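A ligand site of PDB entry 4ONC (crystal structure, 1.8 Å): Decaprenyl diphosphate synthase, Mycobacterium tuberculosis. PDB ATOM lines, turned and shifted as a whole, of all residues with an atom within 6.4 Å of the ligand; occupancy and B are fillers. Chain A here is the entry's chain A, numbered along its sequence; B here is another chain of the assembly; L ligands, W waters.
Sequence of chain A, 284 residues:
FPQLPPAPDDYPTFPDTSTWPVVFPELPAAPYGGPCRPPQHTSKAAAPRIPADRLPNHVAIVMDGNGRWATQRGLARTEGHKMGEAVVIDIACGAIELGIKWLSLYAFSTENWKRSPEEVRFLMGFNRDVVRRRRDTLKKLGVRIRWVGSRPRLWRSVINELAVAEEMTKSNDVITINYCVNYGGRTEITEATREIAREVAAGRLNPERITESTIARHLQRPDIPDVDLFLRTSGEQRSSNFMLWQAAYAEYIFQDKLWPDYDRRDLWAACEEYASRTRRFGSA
NE of Arg 77 is in salt-bridge range of O4 of the ligand, 2.7 Å away. The backbone NH (N) of Arg 68 is in hydrogen-bond range of an oxygen (O5) of the ligand (2.6 Å). The backbone NH (N) of Gly 67 is in hydrogen-bond range of an oxygen (O4) of the ligand (2.8 Å). The guanidinium group (NE) of Arg 68 is in salt-bridge range of an oxygen (O5) of the ligand (2.8 Å). O1 of the ligand lies within hydrogen-bond range of N of Phe 281 of chain B, 3.1 Å away. An oxygen (O2) of the ligand lies within salt-bridge range of the guanidinium group of Arg 115 (2.6 Å).
The guanidinium group (NE) of Arg 280 of chain B lies within salt-bridge range of the side-chain carboxylate (OE2) of Glu 236. The guanidinium group of Arg 68 lies within salt-bridge range of the side-chain carboxylate of Glu 236. O of Gly 67 lies within hydrogen-bond range of OG1 of Thr 71, at 2.7 Å. NH2 of Arg 68 lies within hydrogen-bond range of OG of Ser 234. NH1 of Arg 77 sits close to NE2 of His 81 (3.4 Å). ND2 of Asn 66 is in hydrogen-bond range of ND1 of His 81, 3.0 Å away.
The backbone carbonyl oxygen (O) of Gly 65 lies close to an oxygen (O5) of the ligand (3.5 Å). Merely in contact with the ligand: Asn 66, Thr 71 and Arg 280 of chain B. Hydrophobic or aromatic side chains within 4 Å of the ligand: Phe 281 of chain B. Within 4 Å of the ligand: Gly 65, Asn 66, Gly 67, Arg 68, Thr 71, Arg 77, Arg 115, Arg 280 of chain B and Phe 281 of chain B. The nearest printed residue that does not touch the ligand is Gln 72 (4.2 Å).
Water W2 lies within hydrogen-bond range of an oxygen (O1) of the ligand (2.8 Å) and the guanidinium group (NH1) of Arg 280 of chain B (3.4 Å). Water W1 bridges an oxygen (O6) of the ligand and the guanidinium group (NH2) of Arg 77. Water W3 lies within hydrogen-bond range of OD2 of Asp 64, O3 of the ligand and NH2 of Arg 68.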
ATOM      1  N   ASP A  64       7.710  -1.903   8.664  1.00  0.00           N
ATOM      2  CA  ASP A  64       7.678  -2.693   7.479  1.00  0.00           C
ATOM      3  C   ASP A  64       8.494  -2.040   6.364  1.00  0.00           C
ATOM      4  O   ASP A  64       8.549  -0.774   6.293  1.00  0.00           O
ATOM      5  CB  ASP A  64       6.223  -2.531   6.978  1.00  0.00           C
ATOM      6  CG  ASP A  64       5.444  -3.820   7.035  1.00  0.00           C
ATOM      7  OD1 ASP A  64       5.647  -4.541   8.015  1.00  0.00           O
ATOM      8  OD2 ASP A  64       4.601  -4.111   6.121  1.00  0.00           O
ATOM      9  N   GLY A  65       8.989  -2.847   5.440  1.00  0.00           N
ATOM     10  CA  GLY A  65       9.672  -2.332   4.268  1.00  0.00           C
ATOM     11  C   GLY A  65      11.200  -2.460   4.210  1.00  0.00           C
ATOM     12  O   GLY A  65      11.838  -1.974   3.251  1.00  0.00           O
ATOM     13  N   ASN A  66      11.814  -3.180   5.133  1.00  0.00           N
ATOM     14  CA  ASN A  66      13.281  -3.230   5.168  1.00  0.00           C
ATOM     15  C   ASN A  66      13.836  -4.001   3.954  1.00  0.00           C
ATOM     16  O   ASN A  66      14.880  -3.633   3.436  1.00  0.00           O
ATOM     17  CB  ASN A  66      13.792  -3.985   6.436  1.00  0.00           C
ATOM     18  CG  ASN A  66      13.603  -3.187   7.695  1.00  0.00           C
ATOM     19  OD1 ASN A  66      13.149  -2.019   7.619  1.00  0.00           O
ATOM     20  ND2 ASN A  66      13.912  -3.802   8.885  1.00  0.00           N
ATOM     21  N   GLY A  67      13.118  -5.036   3.460  1.00  0.00           N
ATOM     22  CA  GLY A  67      13.661  -5.760   2.299  1.00  0.00           C
ATOM     23  C   GLY A  67      13.411  -4.988   1.006  1.00  0.00           C
ATOM     24  O   GLY A  67      14.258  -5.033   0.139  1.00  0.00           O
ATOM     25  N   ARG A  68      12.272  -4.334   0.817  1.00  0.00           N
ATOM     26  CA  ARG A  68      12.060  -3.544  -0.408  1.00  0.00           C
ATOM     27  C   ARG A  68      13.142  -2.498  -0.447  1.00  0.00           C
ATOM     28  O   ARG A  68      13.668  -2.174  -1.489  1.00  0.00           O
ATOM     29  CB  ARG A  68      10.694  -2.861  -0.493  1.00  0.00           C
ATOM     30  CG  ARG A  68       9.639  -3.760  -1.053  1.00  0.00           C
ATOM     31  CD  ARG A  68       8.223  -3.299  -0.617  1.00  0.00           C
ATOM     32  NE  ARG A  68       7.941  -3.803   0.746  1.00  0.00           N
ATOM     33  CZ  ARG A  68       6.827  -3.478   1.416  1.00  0.00           C
ATOM     34  NH1 ARG A  68       5.956  -2.571   0.863  1.00  0.00           N
ATOM     35  NH2 ARG A  68       6.641  -3.975   2.626  1.00  0.00           N
ATOM     36  N   TRP A  69      13.464  -1.929   0.738  1.00  0.00           N
ATOM     37  CA  TRP A  69      14.455  -0.876   0.811  1.00  0.00           C
ATOM     38  C   TRP A  69      15.803  -1.406   0.380  1.00  0.00           C
ATOM     39  O   TRP A  69      16.535  -0.784  -0.406  1.00  0.00           O
ATOM     40  CB  TRP A  69      14.455  -0.324   2.302  1.00  0.00           C
ATOM     41  CG  TRP A  69      15.453   0.796   2.439  1.00  0.00           C
ATOM     42  CD1 TRP A  69      15.241   2.167   2.309  1.00  0.00           C
ATOM     43  CD2 TRP A  69      16.885   0.638   2.766  1.00  0.00           C
ATOM     44  NE1 TRP A  69      16.407   2.842   2.540  1.00  0.00           N
ATOM     45  CE2 TRP A  69      17.440   1.975   2.801  1.00  0.00           C
ATOM     46  CE3 TRP A  69      17.715  -0.478   2.968  1.00  0.00           C
ATOM     47  CZ2 TRP A  69      18.790   2.211   3.020  1.00  0.00           C
ATOM     48  CZ3 TRP A  69      19.077  -0.248   3.205  1.00  0.00           C
ATOM     49  CH2 TRP A  69      19.591   1.072   3.238  1.00  0.00           C
ATOM     50  N   THR A  71      16.391  -4.115  -1.393  1.00  0.00           N
ATOM     51  CA  THR A  71      16.320  -4.542  -2.804  1.00  0.00           C
ATOM     52  C   THR A  71      16.510  -3.393  -3.809  1.00  0.00           C
ATOM     53  O   THR A  71      17.211  -3.538  -4.816  1.00  0.00           O
ATOM     54  CB  THR A  71      14.990  -5.239  -3.081  1.00  0.00           C
ATOM     55  OG1 THR A  71      14.854  -6.298  -2.152  1.00  0.00           O
ATOM     56  CG2 THR A  71      14.974  -5.781  -4.495  1.00  0.00           C
ATOM     57  N   GLN A  72      15.939  -2.240  -3.520  1.00  0.00           N
ATOM     58  CA  GLN A  72      16.143  -1.128  -4.388  1.00  0.00           C
ATOM     59  C   GLN A  72      17.623  -0.785  -4.502  1.00  0.00           C
ATOM     60  O   GLN A  72      18.045  -0.244  -5.523  1.00  0.00           O
ATOM     61  CB  GLN A  72      15.332   0.095  -3.866  1.00  0.00           C
ATOM     62  CG  GLN A  72      13.851  -0.220  -3.990  1.00  0.00           C
ATOM     63  CD  GLN A  72      12.912   0.736  -3.276  1.00  0.00           C
ATOM     64  OE1 GLN A  72      13.277   1.856  -2.898  1.00  0.00           O
ATOM     65  NE2 GLN A  72      11.660   0.299  -3.106  1.00  0.00           N
ATOM     66  N   ARG A  77      18.424  -8.284   2.568  1.00  0.00           N
ATOM     67  CA  ARG A  77      17.437  -7.749   3.500  1.00  0.00           C
ATOM     68  C   ARG A  77      18.085  -7.377   4.838  1.00  0.00           C
ATOM     69  O   ARG A  77      17.652  -6.402   5.510  1.00  0.00           O
ATOM     70  CB  ARG A  77      16.244  -8.711   3.692  1.00  0.00           C
ATOM     71  CG  ARG A  77      15.057  -8.150   4.495  1.00  0.00           C
ATOM     72  CD  ARG A  77      13.890  -9.137   4.436  1.00  0.00           C
ATOM     73  NE  ARG A  77      12.633  -8.488   4.869  1.00  0.00           N
ATOM     74  CZ  ARG A  77      11.993  -8.782   5.995  1.00  0.00           C
ATOM     75  NH1 ARG A  77      12.483  -9.747   6.812  1.00  0.00           N
ATOM     76  NH2 ARG A  77      10.837  -8.112   6.270  1.00  0.00           N
ATOM     77  N   HIS A  81      17.452  -4.298   7.762  1.00  0.00           N
ATOM     78  CA  HIS A  81      17.346  -4.449   9.210  1.00  0.00           C
ATOM     79  C   HIS A  81      18.336  -3.618   9.920  1.00  0.00           C
ATOM     80  O   HIS A  81      17.965  -2.967  10.905  1.00  0.00           O
ATOM     81  CB  HIS A  81      17.554  -5.905   9.615  1.00  0.00           C
ATOM     82  CG  HIS A  81      16.533  -6.840   9.055  1.00  0.00           C
ATOM     83  ND1 HIS A  81      15.203  -6.529   9.004  1.00  0.00           N
ATOM     84  CD2 HIS A  81      16.661  -8.102   8.495  1.00  0.00           C
ATOM     85  CE1 HIS A  81      14.507  -7.552   8.473  1.00  0.00           C
ATOM     86  NE2 HIS A  81      15.400  -8.507   8.128  1.00  0.00           N
ATOM     87  N   ARG A 115      10.496 -17.443   7.700  1.00  0.00           N
ATOM     88  CA  ARG A 115      11.553 -16.857   6.866  1.00  0.00           C
ATOM     89  C   ARG A 115      12.732 -17.843   6.726  1.00  0.00           C
ATOM     90  O   ARG A 115      12.736 -18.886   7.390  1.00  0.00           O
ATOM     91  CB  ARG A 115      12.021 -15.515   7.378  1.00  0.00           C
ATOM     92  CG  ARG A 115      10.865 -14.508   7.121  1.00  0.00           C
ATOM     93  CD  ARG A 115      11.281 -13.105   7.341  1.00  0.00           C
ATOM     94  NE  ARG A 115      10.096 -12.268   7.272  1.00  0.00           N
ATOM     95  CZ  ARG A 115       9.673 -11.568   6.210  1.00  0.00           C
ATOM     96  NH1 ARG A 115      10.327 -11.522   5.066  1.00  0.00           N
ATOM     97  NH2 ARG A 115       8.593 -10.859   6.336  1.00  0.00           N
ATOM     98  N   SER A 234       5.424   1.308   4.657  1.00  0.00           N
ATOM     99  CA  SER A 234       5.568   0.567   3.405  1.00  0.00           C
ATOM    100  C   SER A 234       4.221   0.423   2.654  1.00  0.00           C
ATOM    101  O   SER A 234       4.164  -0.248   1.649  1.00  0.00           O
ATOM    102  CB  SER A 234       6.297  -0.769   3.528  1.00  0.00           C
ATOM    103  OG  SER A 234       5.346  -1.837   3.891  1.00  0.00           O
ATOM    104  N   GLU A 236       1.459  -0.897   3.698  1.00  0.00           N
ATOM    105  CA  GLU A 236       0.743  -2.200   3.897  1.00  0.00           C
ATOM    106  C   GLU A 236      -0.430  -1.820   4.826  1.00  0.00           C
ATOM    107  O   GLU A 236      -0.185  -1.095   5.792  1.00  0.00           O
ATOM    108  CB  GLU A 236       1.610  -3.214   4.708  1.00  0.00           C
ATOM    109  CG  GLU A 236       2.689  -3.906   3.873  1.00  0.00           C
ATOM    110  CD  GLU A 236       2.194  -4.369   2.494  1.00  0.00           C
ATOM    111  OE1 GLU A 236       1.260  -5.228   2.429  1.00  0.00           O
ATOM    112  OE2 GLU A 236       2.762  -3.831   1.480  1.00  0.00           O
ATOM    113  N   ARG A 238      -2.591  -3.629   7.023  1.00  0.00           N
ATOM    114  CA  ARG A 238      -2.956  -4.836   7.836  1.00  0.00           C
ATOM    115  C   ARG A 238      -2.438  -4.588   9.233  1.00  0.00           C
ATOM    116  O   ARG A 238      -1.440  -3.833   9.407  1.00  0.00           O
ATOM    117  CB  ARG A 238      -2.209  -6.069   7.313  1.00  0.00           C
ATOM    118  CG  ARG A 238      -2.736  -6.500   5.995  1.00  0.00           C
ATOM    119  CD  ARG A 238      -2.272  -7.871   5.512  1.00  0.00           C
ATOM    120  NE  ARG A 238      -0.863  -8.125   5.743  1.00  0.00           N
ATOM    121  CZ  ARG A 238       0.183  -7.590   5.096  1.00  0.00           C
ATOM    122  NH1 ARG A 238       0.019  -6.677   4.139  1.00  0.00           N
ATOM    123  NH2 ARG A 238       1.436  -7.991   5.426  1.00  0.00           N
ATOM    124  N   LEU A 258       9.140   3.470   3.395  1.00  0.00           N
ATOM    125  CA  LEU A 258       9.743   2.242   3.865  1.00  0.00           C
ATOM    126  C   LEU A 258      10.462   2.509   5.178  1.00  0.00           C
ATOM    127  O   LEU A 258      10.989   3.641   5.411  1.00  0.00           O
ATOM    128  CB  LEU A 258      10.781   1.731   2.872  1.00  0.00           C
ATOM    129  CG  LEU A 258      10.166   1.553   1.441  1.00  0.00           C
ATOM    130  CD1 LEU A 258      11.347   1.048   0.567  1.00  0.00           C
ATOM    131  CD2 LEU A 258       9.096   0.482   1.444  1.00  0.00           C
ATOM    132  N   ARG B 279       0.696  -9.690  -2.633  1.00  0.00           N
ATOM    133  CA  ARG B 279       0.625 -10.467  -1.433  1.00  0.00           C
ATOM    134  C   ARG B 279       2.032 -10.713  -0.998  1.00  0.00           C
ATOM    135  O   ARG B 279       2.806 -11.355  -1.702  1.00  0.00           O
ATOM    136  CB  ARG B 279      -0.112 -11.784  -1.713  1.00  0.00           C
ATOM    137  CG  ARG B 279      -1.486 -11.537  -2.340  1.00  0.00           C
ATOM    138  CD  ARG B 279      -2.594 -11.526  -1.291  1.00  0.00           C
ATOM    139  NE  ARG B 279      -3.888 -11.756  -1.943  1.00  0.00           N
ATOM    140  CZ  ARG B 279      -4.619 -10.831  -2.550  1.00  0.00           C
ATOM    141  NH1 ARG B 279      -4.213  -9.515  -2.593  1.00  0.00           N
ATOM    142  NH2 ARG B 279      -5.750 -11.225  -3.118  1.00  0.00           N
ATOM    143  N   ARG B 280       2.364 -10.260   0.185  1.00  0.00           N
ATOM    144  CA  ARG B 280       3.777 -10.271   0.622  1.00  0.00           C
ATOM    145  C   ARG B 280       4.212 -11.623   1.265  1.00  0.00           C
ATOM    146  O   ARG B 280       3.385 -12.531   1.444  1.00  0.00           O
ATOM    147  CB  ARG B 280       4.025  -9.087   1.572  1.00  0.00           C
ATOM    148  CG  ARG B 280       3.566  -7.778   0.914  1.00  0.00           C
ATOM    149  CD  ARG B 280       4.646  -6.723   0.829  1.00  0.00           C
ATOM    150  NE  ARG B 280       4.142  -5.549   0.078  1.00  0.00           N
ATOM    151  CZ  ARG B 280       4.588  -5.115  -1.114  1.00  0.00           C
ATOM    152  NH1 ARG B 280       5.622  -5.712  -1.742  1.00  0.00           N
ATOM    153  NH2 ARG B 280       4.002  -4.064  -1.691  1.00  0.00           N
ATOM    154  N   PHE B 281       5.500 -11.700   1.634  1.00  0.00           N
ATOM    155  CA  PHE B 281       6.102 -12.963   2.023  1.00  0.00           C
ATOM    156  C   PHE B 281       5.248 -13.529   3.166  1.00  0.00           C
ATOM    157  O   PHE B 281       4.903 -12.813   4.116  1.00  0.00           O
ATOM    158  CB  PHE B 281       7.522 -12.775   2.563  1.00  0.00           C
ATOM    159  CG  PHE B 281       8.091 -14.077   3.102  1.00  0.00           C
ATOM    160  CD1 PHE B 281       8.649 -15.023   2.207  1.00  0.00           C
ATOM    161  CD2 PHE B 281       8.008 -14.377   4.464  1.00  0.00           C
ATOM    162  CE1 PHE B 281       9.155 -16.208   2.700  1.00  0.00           C
ATOM    163  CE2 PHE B 281       8.487 -15.588   4.944  1.00  0.00           C
ATOM    164  CZ  PHE B 281       9.097 -16.475   4.067  1.00  0.00           C
ATOM    165  N   GLY B 282       4.934 -14.798   3.074  1.00  0.00           N
ATOM    166  CA  GLY B 282       4.292 -15.566   4.124  1.00  0.00           C
ATOM    167  C   GLY B 282       2.777 -15.319   4.248  1.00  0.00           C
ATOM    168  O   GLY B 282       2.109 -15.946   5.064  1.00  0.00           O
HETATM  169  O1  LIG L   1       7.752  -9.682   1.062  1.00  0.00           O
HETATM  170  P1  LIG L   1       8.324  -8.908   2.417  1.00  0.00           P
HETATM  171  O2  LIG L   1       9.260  -9.854   3.313  1.00  0.00           O
HETATM  172  O3  LIG L   1       7.197  -8.446   3.266  1.00  0.00           O
HETATM  173  C1  LIG L   1       9.280  -7.471   1.662  1.00  0.00           C
HETATM  174  P2  LIG L   1       9.779  -6.162   3.005  1.00  0.00           P
HETATM  175  O4  LIG L   1      10.875  -6.594   4.002  1.00  0.00           O
HETATM  176  O5  LIG L   1      10.124  -4.803   2.173  1.00  0.00           O
HETATM  177  O6  LIG L   1       8.420  -5.930   3.727  1.00  0.00           O
HETATM  178  O7  LIG L   1       8.335  -6.778   0.776  1.00  0.00           O
HETATM  179  C2  LIG L   1      10.458  -7.879   0.906  1.00  0.00           C
HETATM  180  C3  LIG L   1      10.470  -7.604  -0.507  1.00  0.00           C
HETATM  181  C4  LIG L   1      11.524  -8.537   1.561  1.00  0.00           C
HETATM  182  C5  LIG L   1      12.650  -8.932   0.764  1.00  0.00           C
HETATM  183  C6  LIG L   1      12.658  -8.684  -0.616  1.00  0.00           C
HETATM  184  C7  LIG L   1      11.580  -8.010  -1.280  1.00  0.00           C
HETATM  185  C8  LIG L   1      11.495  -7.823  -2.709  1.00  0.00           C
HETATM  186  C9  LIG L   1      11.106  -6.633  -3.364  1.00  0.00           C
HETATM  187  C10 LIG L   1      11.701  -8.980  -3.523  1.00  0.00           C
HETATM  188  C11 LIG L   1      11.602  -8.955  -4.932  1.00  0.00           C
HETATM  189  C12 LIG L   1      11.221  -7.753  -5.567  1.00  0.00           C
HETATM  190  C13 LIG L   1      10.986  -6.581  -4.785  1.00  0.00           C
HETATM  191  C14 LIG L   1      10.615  -5.376  -5.447  1.00  0.00           C
HETATM  192  C15 LIG L   1       9.841  -5.438  -6.632  1.00  0.00           C
HETATM  193  C16 LIG L   1       9.450  -4.253  -7.303  1.00  0.00           C
HETATM  194  C17 LIG L   1       9.852  -3.011  -6.760  1.00  0.00           C
HETATM  195  C18 LIG L   1      10.628  -2.930  -5.587  1.00  0.00           C
HETATM  196  C19 LIG L   1      11.003  -4.111  -4.921  1.00  0.00           C
HETATM  197  O   HOH W   1       8.568  -6.171   6.670  1.00  0.00           O
HETATM  198  O   HOH W   2       6.886  -8.809  -1.491  1.00  0.00           O
HETATM  199  O   HOH W   3       5.014  -6.500   4.341  1.00  0.00           O
